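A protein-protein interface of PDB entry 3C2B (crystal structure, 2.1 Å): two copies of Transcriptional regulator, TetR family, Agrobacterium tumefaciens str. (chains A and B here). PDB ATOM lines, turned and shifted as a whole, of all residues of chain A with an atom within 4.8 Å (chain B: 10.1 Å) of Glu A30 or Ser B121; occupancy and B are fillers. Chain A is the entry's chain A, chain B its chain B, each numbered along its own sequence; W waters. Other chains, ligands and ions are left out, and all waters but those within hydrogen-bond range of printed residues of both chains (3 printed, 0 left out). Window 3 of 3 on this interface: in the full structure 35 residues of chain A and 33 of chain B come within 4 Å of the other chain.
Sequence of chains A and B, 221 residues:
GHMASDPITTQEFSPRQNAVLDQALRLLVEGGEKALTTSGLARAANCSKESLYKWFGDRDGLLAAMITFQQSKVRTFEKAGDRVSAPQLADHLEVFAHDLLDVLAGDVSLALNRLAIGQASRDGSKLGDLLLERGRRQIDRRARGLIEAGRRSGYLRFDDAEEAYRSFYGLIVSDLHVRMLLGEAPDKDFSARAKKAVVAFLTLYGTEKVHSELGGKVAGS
Water W2 bridges O of Glu A30 (2.5 Å) and OD2 of Asp B123 (2.7 Å). Water W1 bridges the backbone carbonyl oxygen (O) of Arg B122 (2.7 Å) and the guanidinium group (NH2) of Arg A114 (2.7 Å). Water W3 lies within hydrogen-bond range of O of Leu A28, NH1 of Arg A114 and O of Ala B120.
No position is printed for both chains. Of the 11 pairs that touch across the chains among the printed residues, none has its exchanged pair printed and touching as well.
The backbone carbonyl oxygen of Val A29 sits at hydrogen-bond distance from the backbone NH of Arg B122 (3.2 Å). The guanidinium group (NH1) of Arg A114 lies close to the backbone carbonyl oxygen (O) of Ser B121. N of Arg B122 sits close to NH1 of Arg A114.
Hydrophobic or aromatic side chains of chain B within 4 Å of the printed part of chain A: Ile B117 and Ala B120.
Of chain B, only Ser B121 (3.6 Å) comes within 4 Å of Glu A30. Of chain A, only Val A29, Glu A30, Gly A31, Gly A32 and Arg A114 come within 4 Å of Ser B121. Of chain B, only Ser B121 (3.8 Å) comes within 4 Å of Gly A31. Of the printed residues of chain A, Gly B118 touches Arg A114. Of the printed residues of chain A, Ala B120 touches Gly A32 (3.5 Å) and Arg A114 (3.5 Å). Of the printed residues of chain A, Ile B117 touches Arg A114 (3.5 Å). Ser B125 touches none of the printed residues of chain A. The nearest printed residue of chain B that does not touch Glu A30 is Asp B123 (4.2 Å).
The guanidinium group of Arg A26 is in salt-bridge range of the side-chain carboxylate of Glu A30, at 3.8 Å. The side-chain hydroxyl (OG) of Ser B121 lies close to the backbone NH (N) of Asp B123 (3.1 Å). The side-chain carboxylate (OD1) of Asp B123 is in salt-bridge range of the guanidinium group (NH2) of Arg B122 (3.8 Å).
Among the printed residues, pairs that only touch across the chains: Arg A114 with Ile B117 (3.5 Å), Arg A114 with Ala B120 (3.5 Å), Gly A32 with Ala B120 (3.5 Å), Glu A30 with Ser B121 (3.6 Å), Arg A114 with Gly B118 (3.6 Å), Gly A32 with Ser B121 (3.6 Å), Val A29 with Ser B121 (3.7 Å) and Gly A31 with Ser B121 (3.8 Å).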
ATOM      1  N   ARG A  26       8.452  -0.562  -6.642  1.00  0.00           N
ATOM      2  CA  ARG A  26       7.485  -1.260  -5.791  1.00  0.00           C
ATOM      3  C   ARG A  26       8.149  -2.276  -4.846  1.00  0.00           C
ATOM      4  O   ARG A  26       7.890  -2.249  -3.642  1.00  0.00           O
ATOM      5  CB  ARG A  26       6.407  -1.939  -6.651  1.00  0.00           C
ATOM      6  CG  ARG A  26       5.544  -2.982  -5.927  1.00  0.00           C
ATOM      7  CD  ARG A  26       4.161  -3.136  -6.579  1.00  0.00           C
ATOM      8  NE  ARG A  26       3.312  -1.962  -6.313  1.00  0.00           N
ATOM      9  CZ  ARG A  26       2.105  -1.739  -6.843  1.00  0.00           C
ATOM     10  NH1 ARG A  26       1.552  -2.607  -7.692  1.00  0.00           N
ATOM     11  NH2 ARG A  26       1.446  -0.631  -6.522  1.00  0.00           N
ATOM     12  N   LEU A  27       8.983  -3.167  -5.393  1.00  0.00           N
ATOM     13  CA  LEU A  27       9.666  -4.193  -4.578  1.00  0.00           C
ATOM     14  C   LEU A  27      10.483  -3.544  -3.477  1.00  0.00           C
ATOM     15  O   LEU A  27      10.517  -4.009  -2.338  1.00  0.00           O
ATOM     16  CB  LEU A  27      10.597  -5.062  -5.431  1.00  0.00           C
ATOM     17  CG  LEU A  27      10.018  -6.247  -6.213  1.00  0.00           C
ATOM     18  CD1 LEU A  27      11.082  -6.795  -7.164  1.00  0.00           C
ATOM     19  CD2 LEU A  27       9.493  -7.361  -5.288  1.00  0.00           C
ATOM     20  N   LEU A  28      11.128  -2.444  -3.835  1.00  0.00           N
ATOM     21  CA  LEU A  28      12.031  -1.735  -2.955  1.00  0.00           C
ATOM     22  C   LEU A  28      11.312  -1.109  -1.738  1.00  0.00           C
ATOM     23  O   LEU A  28      11.774  -1.243  -0.605  1.00  0.00           O
ATOM     24  CB  LEU A  28      12.762  -0.671  -3.788  1.00  0.00           C
ATOM     25  CG  LEU A  28      14.236  -0.252  -3.590  1.00  0.00           C
ATOM     26  CD1 LEU A  28      14.313   1.190  -3.289  1.00  0.00           C
ATOM     27  CD2 LEU A  28      15.043  -1.114  -2.625  1.00  0.00           C
ATOM     28  N   VAL A  29      10.191  -0.431  -1.986  1.00  0.00           N
ATOM     29  CA  VAL A  29       9.368   0.150  -0.915  1.00  0.00           C
ATOM     30  C   VAL A  29       8.886  -0.963   0.031  1.00  0.00           C
ATOM     31  O   VAL A  29       8.936  -0.841   1.254  1.00  0.00           O
ATOM     32  CB  VAL A  29       8.156   0.941  -1.489  1.00  0.00           C
ATOM     33  CG1 VAL A  29       7.209   1.444  -0.364  1.00  0.00           C
ATOM     34  CG2 VAL A  29       8.632   2.102  -2.406  1.00  0.00           C
ATOM     35  N   GLU A  30       8.431  -2.055  -0.561  1.00  0.00           N
ATOM     36  CA  GLU A  30       7.788  -3.142   0.195  1.00  0.00           C
ATOM     37  C   GLU A  30       8.751  -4.018   1.039  1.00  0.00           C
ATOM     38  O   GLU A  30       8.472  -4.319   2.207  1.00  0.00           O
ATOM     39  CB  GLU A  30       6.918  -3.964  -0.757  1.00  0.00           C
ATOM     40  CG  GLU A  30       5.797  -3.082  -1.318  1.00  0.00           C
ATOM     41  CD  GLU A  30       4.857  -3.781  -2.269  1.00  0.00           C
ATOM     42  OE1 GLU A  30       5.067  -4.971  -2.588  1.00  0.00           O
ATOM     43  OE2 GLU A  30       3.890  -3.122  -2.708  1.00  0.00           O
ATOM     44  N   GLY A  31       9.889  -4.391   0.457  1.00  0.00           N
ATOM     45  CA  GLY A  31      10.841  -5.244   1.143  1.00  0.00           C
ATOM     46  C   GLY A  31      12.263  -4.728   1.305  1.00  0.00           C
ATOM     47  O   GLY A  31      13.122  -5.467   1.757  1.00  0.00           O
ATOM     48  N   GLY A  32      12.531  -3.477   0.948  1.00  0.00           N
ATOM     49  CA  GLY A  32      13.904  -2.942   1.043  1.00  0.00           C
ATOM     50  C   GLY A  32      14.874  -3.567   0.038  1.00  0.00           C
ATOM     51  O   GLY A  32      14.465  -4.302  -0.889  1.00  0.00           O
ATOM     52  N   ARG A 114      17.283   4.841   1.271  1.00  0.00           N
ATOM     53  CA  ARG A 114      17.709   3.631   1.972  1.00  0.00           C
ATOM     54  C   ARG A 114      18.605   2.775   1.096  1.00  0.00           C
ATOM     55  O   ARG A 114      19.633   2.287   1.546  1.00  0.00           O
ATOM     56  CB  ARG A 114      16.513   2.777   2.383  1.00  0.00           C
ATOM     57  CG  ARG A 114      15.680   3.397   3.480  1.00  0.00           C
ATOM     58  CD  ARG A 114      14.437   2.564   3.787  1.00  0.00           C
ATOM     59  NE  ARG A 114      13.648   3.248   4.816  1.00  0.00           N
ATOM     60  CZ  ARG A 114      12.346   3.484   4.688  1.00  0.00           C
ATOM     61  NH1 ARG A 114      11.679   3.035   3.613  1.00  0.00           N
ATOM     62  NH2 ARG A 114      11.711   4.139   5.629  1.00  0.00           N
ATOM     63  N   LEU B 115      23.836   0.283   8.125  1.00  0.00           N
ATOM     64  CA  LEU B 115      23.275  -1.070   8.206  1.00  0.00           C
ATOM     65  C   LEU B 115      21.764  -0.981   8.483  1.00  0.00           C
ATOM     66  O   LEU B 115      20.978  -1.591   7.749  1.00  0.00           O
ATOM     67  CB  LEU B 115      23.978  -1.959   9.229  1.00  0.00           C
ATOM     68  CG  LEU B 115      23.353  -3.368   9.435  1.00  0.00           C
ATOM     69  CD1 LEU B 115      23.095  -4.199   8.129  1.00  0.00           C
ATOM     70  CD2 LEU B 115      24.111  -4.193  10.458  1.00  0.00           C
ATOM     71  N   ALA B 116      21.365  -0.193   9.489  1.00  0.00           N
ATOM     72  CA  ALA B 116      19.977  -0.189   9.897  1.00  0.00           C
ATOM     73  C   ALA B 116      19.108   0.395   8.767  1.00  0.00           C
ATOM     74  O   ALA B 116      18.024  -0.098   8.487  1.00  0.00           O
ATOM     75  CB  ALA B 116      19.794   0.596  11.166  1.00  0.00           C
ATOM     76  N   ILE B 117      19.605   1.448   8.131  1.00  0.00           N
ATOM     77  CA  ILE B 117      18.889   2.095   7.061  1.00  0.00           C
ATOM     78  C   ILE B 117      18.886   1.244   5.795  1.00  0.00           C
ATOM     79  O   ILE B 117      17.853   1.148   5.135  1.00  0.00           O
ATOM     80  CB  ILE B 117      19.463   3.485   6.775  1.00  0.00           C
ATOM     81  CG1 ILE B 117      19.136   4.408   7.964  1.00  0.00           C
ATOM     82  CG2 ILE B 117      18.925   4.027   5.420  1.00  0.00           C
ATOM     83  CD1 ILE B 117      19.752   5.798   7.875  1.00  0.00           C
ATOM     84  N   GLY B 118      20.031   0.637   5.477  1.00  0.00           N
ATOM     85  CA  GLY B 118      20.221  -0.067   4.223  1.00  0.00           C
ATOM     86  C   GLY B 118      19.290  -1.260   4.164  1.00  0.00           C
ATOM     87  O   GLY B 118      18.921  -1.731   3.071  1.00  0.00           O
ATOM     88  N   GLN B 119      18.900  -1.747   5.345  1.00  0.00           N
ATOM     89  CA  GLN B 119      18.123  -2.977   5.418  1.00  0.00           C
ATOM     90  C   GLN B 119      16.664  -2.683   5.673  1.00  0.00           C
ATOM     91  O   GLN B 119      15.828  -3.575   5.539  1.00  0.00           O
ATOM     92  CB  GLN B 119      18.700  -3.947   6.449  1.00  0.00           C
ATOM     93  CG  GLN B 119      18.562  -3.561   7.919  1.00  0.00           C
ATOM     94  CD  GLN B 119      19.110  -4.648   8.837  1.00  0.00           C
ATOM     95  OE1 GLN B 119      19.230  -4.465  10.059  1.00  0.00           O
ATOM     96  NE2 GLN B 119      19.453  -5.797   8.247  1.00  0.00           N
ATOM     97  N   ALA B 120      16.355  -1.422   5.989  1.00  0.00           N
ATOM     98  CA  ALA B 120      14.974  -1.038   6.221  1.00  0.00           C
ATOM     99  C   ALA B 120      14.080  -1.114   4.971  1.00  0.00           C
ATOM    100  O   ALA B 120      14.526  -0.928   3.833  1.00  0.00           O
ATOM    101  CB  ALA B 120      14.916   0.375   6.830  1.00  0.00           C
ATOM    102  N   SER B 121      12.811  -1.413   5.206  1.00  0.00           N
ATOM    103  CA  SER B 121      11.772  -1.169   4.215  1.00  0.00           C
ATOM    104  C   SER B 121      10.924  -0.030   4.757  1.00  0.00           C
ATOM    105  O   SER B 121      11.249   0.545   5.794  1.00  0.00           O
ATOM    106  CB  SER B 121      10.896  -2.420   4.033  1.00  0.00           C
ATOM    107  OG  SER B 121      10.263  -2.721   5.252  1.00  0.00           O
ATOM    108  N   ARG B 122       9.849   0.307   4.055  1.00  0.00           N
ATOM    109  CA  ARG B 122       8.796   1.145   4.604  1.00  0.00           C
ATOM    110  C   ARG B 122       8.519   0.848   6.091  1.00  0.00           C
ATOM    111  O   ARG B 122       8.171   1.748   6.865  1.00  0.00           O
ATOM    112  CB  ARG B 122       7.508   0.960   3.788  1.00  0.00           C
ATOM    113  CG  ARG B 122       6.249   1.483   4.487  1.00  0.00           C
ATOM    114  CD  ARG B 122       5.200   1.907   3.493  1.00  0.00           C
ATOM    115  NE  ARG B 122       3.978   2.386   4.129  1.00  0.00           N
ATOM    116  CZ  ARG B 122       3.119   1.618   4.802  1.00  0.00           C
ATOM    117  NH1 ARG B 122       2.019   2.153   5.320  1.00  0.00           N
ATOM    118  NH2 ARG B 122       3.358   0.321   4.974  1.00  0.00           N
ATOM    119  N   ASP B 123       8.673  -0.419   6.473  1.00  0.00           N
ATOM    120  CA  ASP B 123       8.406  -0.938   7.813  1.00  0.00           C
ATOM    121  C   ASP B 123       9.607  -0.885   8.760  1.00  0.00           C
ATOM    122  O   ASP B 123       9.556  -1.460   9.844  1.00  0.00           O
ATOM    123  CB  ASP B 123       7.945  -2.403   7.711  1.00  0.00           C
ATOM    124  CG  ASP B 123       6.715  -2.575   6.855  1.00  0.00           C
ATOM    125  OD1 ASP B 123       5.733  -1.831   7.068  1.00  0.00           O
ATOM    126  OD2 ASP B 123       6.733  -3.469   5.980  1.00  0.00           O
ATOM    127  N   GLY B 124      10.703  -0.262   8.335  1.00  0.00           N
ATOM    128  CA  GLY B 124      11.912  -0.179   9.176  1.00  0.00           C
ATOM    129  C   GLY B 124      12.703  -1.459   9.222  1.00  0.00           C
ATOM    130  O   GLY B 124      12.640  -2.245   8.298  1.00  0.00           O
ATOM    131  N   SER B 125      13.431  -1.655  10.314  1.00  0.00           N
ATOM    132  CA  SER B 125      14.188  -2.868  10.595  1.00  0.00           C
ATOM    133  C   SER B 125      14.352  -2.933  12.106  1.00  0.00           C
ATOM    134  O   SER B 125      14.144  -1.952  12.790  1.00  0.00           O
ATOM    135  CB  SER B 125      15.558  -2.801   9.943  1.00  0.00           C
ATOM    136  OG  SER B 125      16.268  -1.664  10.428  1.00  0.00           O
ATOM    137  N   LYS B 126      14.711  -4.089  12.620  1.00  0.00           N
ATOM    138  CA  LYS B 126      14.927  -4.267  14.061  1.00  0.00           C
ATOM    139  C   LYS B 126      16.061  -3.379  14.621  1.00  0.00           C
ATOM    140  O   LYS B 126      15.894  -2.732  15.669  1.00  0.00           O
ATOM    141  CB  LYS B 126      15.189  -5.743  14.382  1.00  0.00           C
ATOM    142  CG  LYS B 126      15.477  -6.005  15.873  1.00  0.00           C
ATOM    143  CD  LYS B 126      14.191  -5.922  16.717  1.00  0.00           C
ATOM    144  CE  LYS B 126      14.481  -5.723  18.210  1.00  0.00           C
ATOM    145  NZ  LYS B 126      13.387  -6.233  19.100  1.00  0.00           N
ATOM    146  N   LEU B 127      17.200  -3.368  13.915  1.00  0.00           N
ATOM    147  CA  LEU B 127      18.302  -2.479  14.237  1.00  0.00           C
ATOM    148  C   LEU B 127      17.856  -1.027  14.198  1.00  0.00           C
ATOM    149  O   LEU B 127      18.242  -0.237  15.042  1.00  0.00           O
ATOM    150  CB  LEU B 127      19.485  -2.696  13.290  1.00  0.00           C
ATOM    151  CG  LEU B 127      20.740  -1.884  13.671  1.00  0.00           C
ATOM    152  CD1 LEU B 127      21.207  -2.165  15.094  1.00  0.00           C
ATOM    153  CD2 LEU B 127      21.854  -2.187  12.696  1.00  0.00           C
ATOM    154  N   GLY B 128      17.039  -0.691  13.207  1.00  0.00           N
ATOM    155  CA  GLY B 128      16.430   0.613  13.134  1.00  0.00           C
ATOM    156  C   GLY B 128      15.667   0.975  14.400  1.00  0.00           C
ATOM    157  O   GLY B 128      15.799   2.099  14.887  1.00  0.00           O
ATOM    158  N   ASP B 129      14.860   0.041  14.915  1.00  0.00           N
ATOM    159  CA  ASP B 129      14.116   0.207  16.175  1.00  0.00           C
ATOM    160  C   ASP B 129      15.071   0.551  17.329  1.00  0.00           C
ATOM    161  O   ASP B 129      14.833   1.511  18.097  1.00  0.00           O
ATOM    162  CB  ASP B 129      13.349  -1.090  16.542  1.00  0.00           C
ATOM    163  CG  ASP B 129      12.234  -1.424  15.557  1.00  0.00           C
ATOM    164  OD1 ASP B 129      11.845  -0.565  14.710  1.00  0.00           O
ATOM    165  OD2 ASP B 129      11.760  -2.575  15.615  1.00  0.00           O
ATOM    166  N   LEU B 132      16.634   4.147  16.948  1.00  0.00           N
ATOM    167  CA  LEU B 132      15.592   5.169  17.218  1.00  0.00           C
ATOM    168  C   LEU B 132      15.376   5.278  18.738  1.00  0.00           C
ATOM    169  O   LEU B 132      15.140   6.366  19.272  1.00  0.00           O
ATOM    170  CB  LEU B 132      14.282   4.757  16.524  1.00  0.00           C
ATOM    171  CG  LEU B 132      13.679   5.366  15.241  1.00  0.00           C
ATOM    172  CD1 LEU B 132      14.418   6.574  14.612  1.00  0.00           C
ATOM    173  CD2 LEU B 132      13.304   4.302  14.208  1.00  0.00           C
HETATM  174  O   HOH W   1       8.997   4.226   6.035  1.00  0.00           O
HETATM  175  O   HOH W   2       6.250  -4.034   3.346  1.00  0.00           O
HETATM  176  O   HOH W   3      12.517   0.565   1.450  1.00  0.00           O
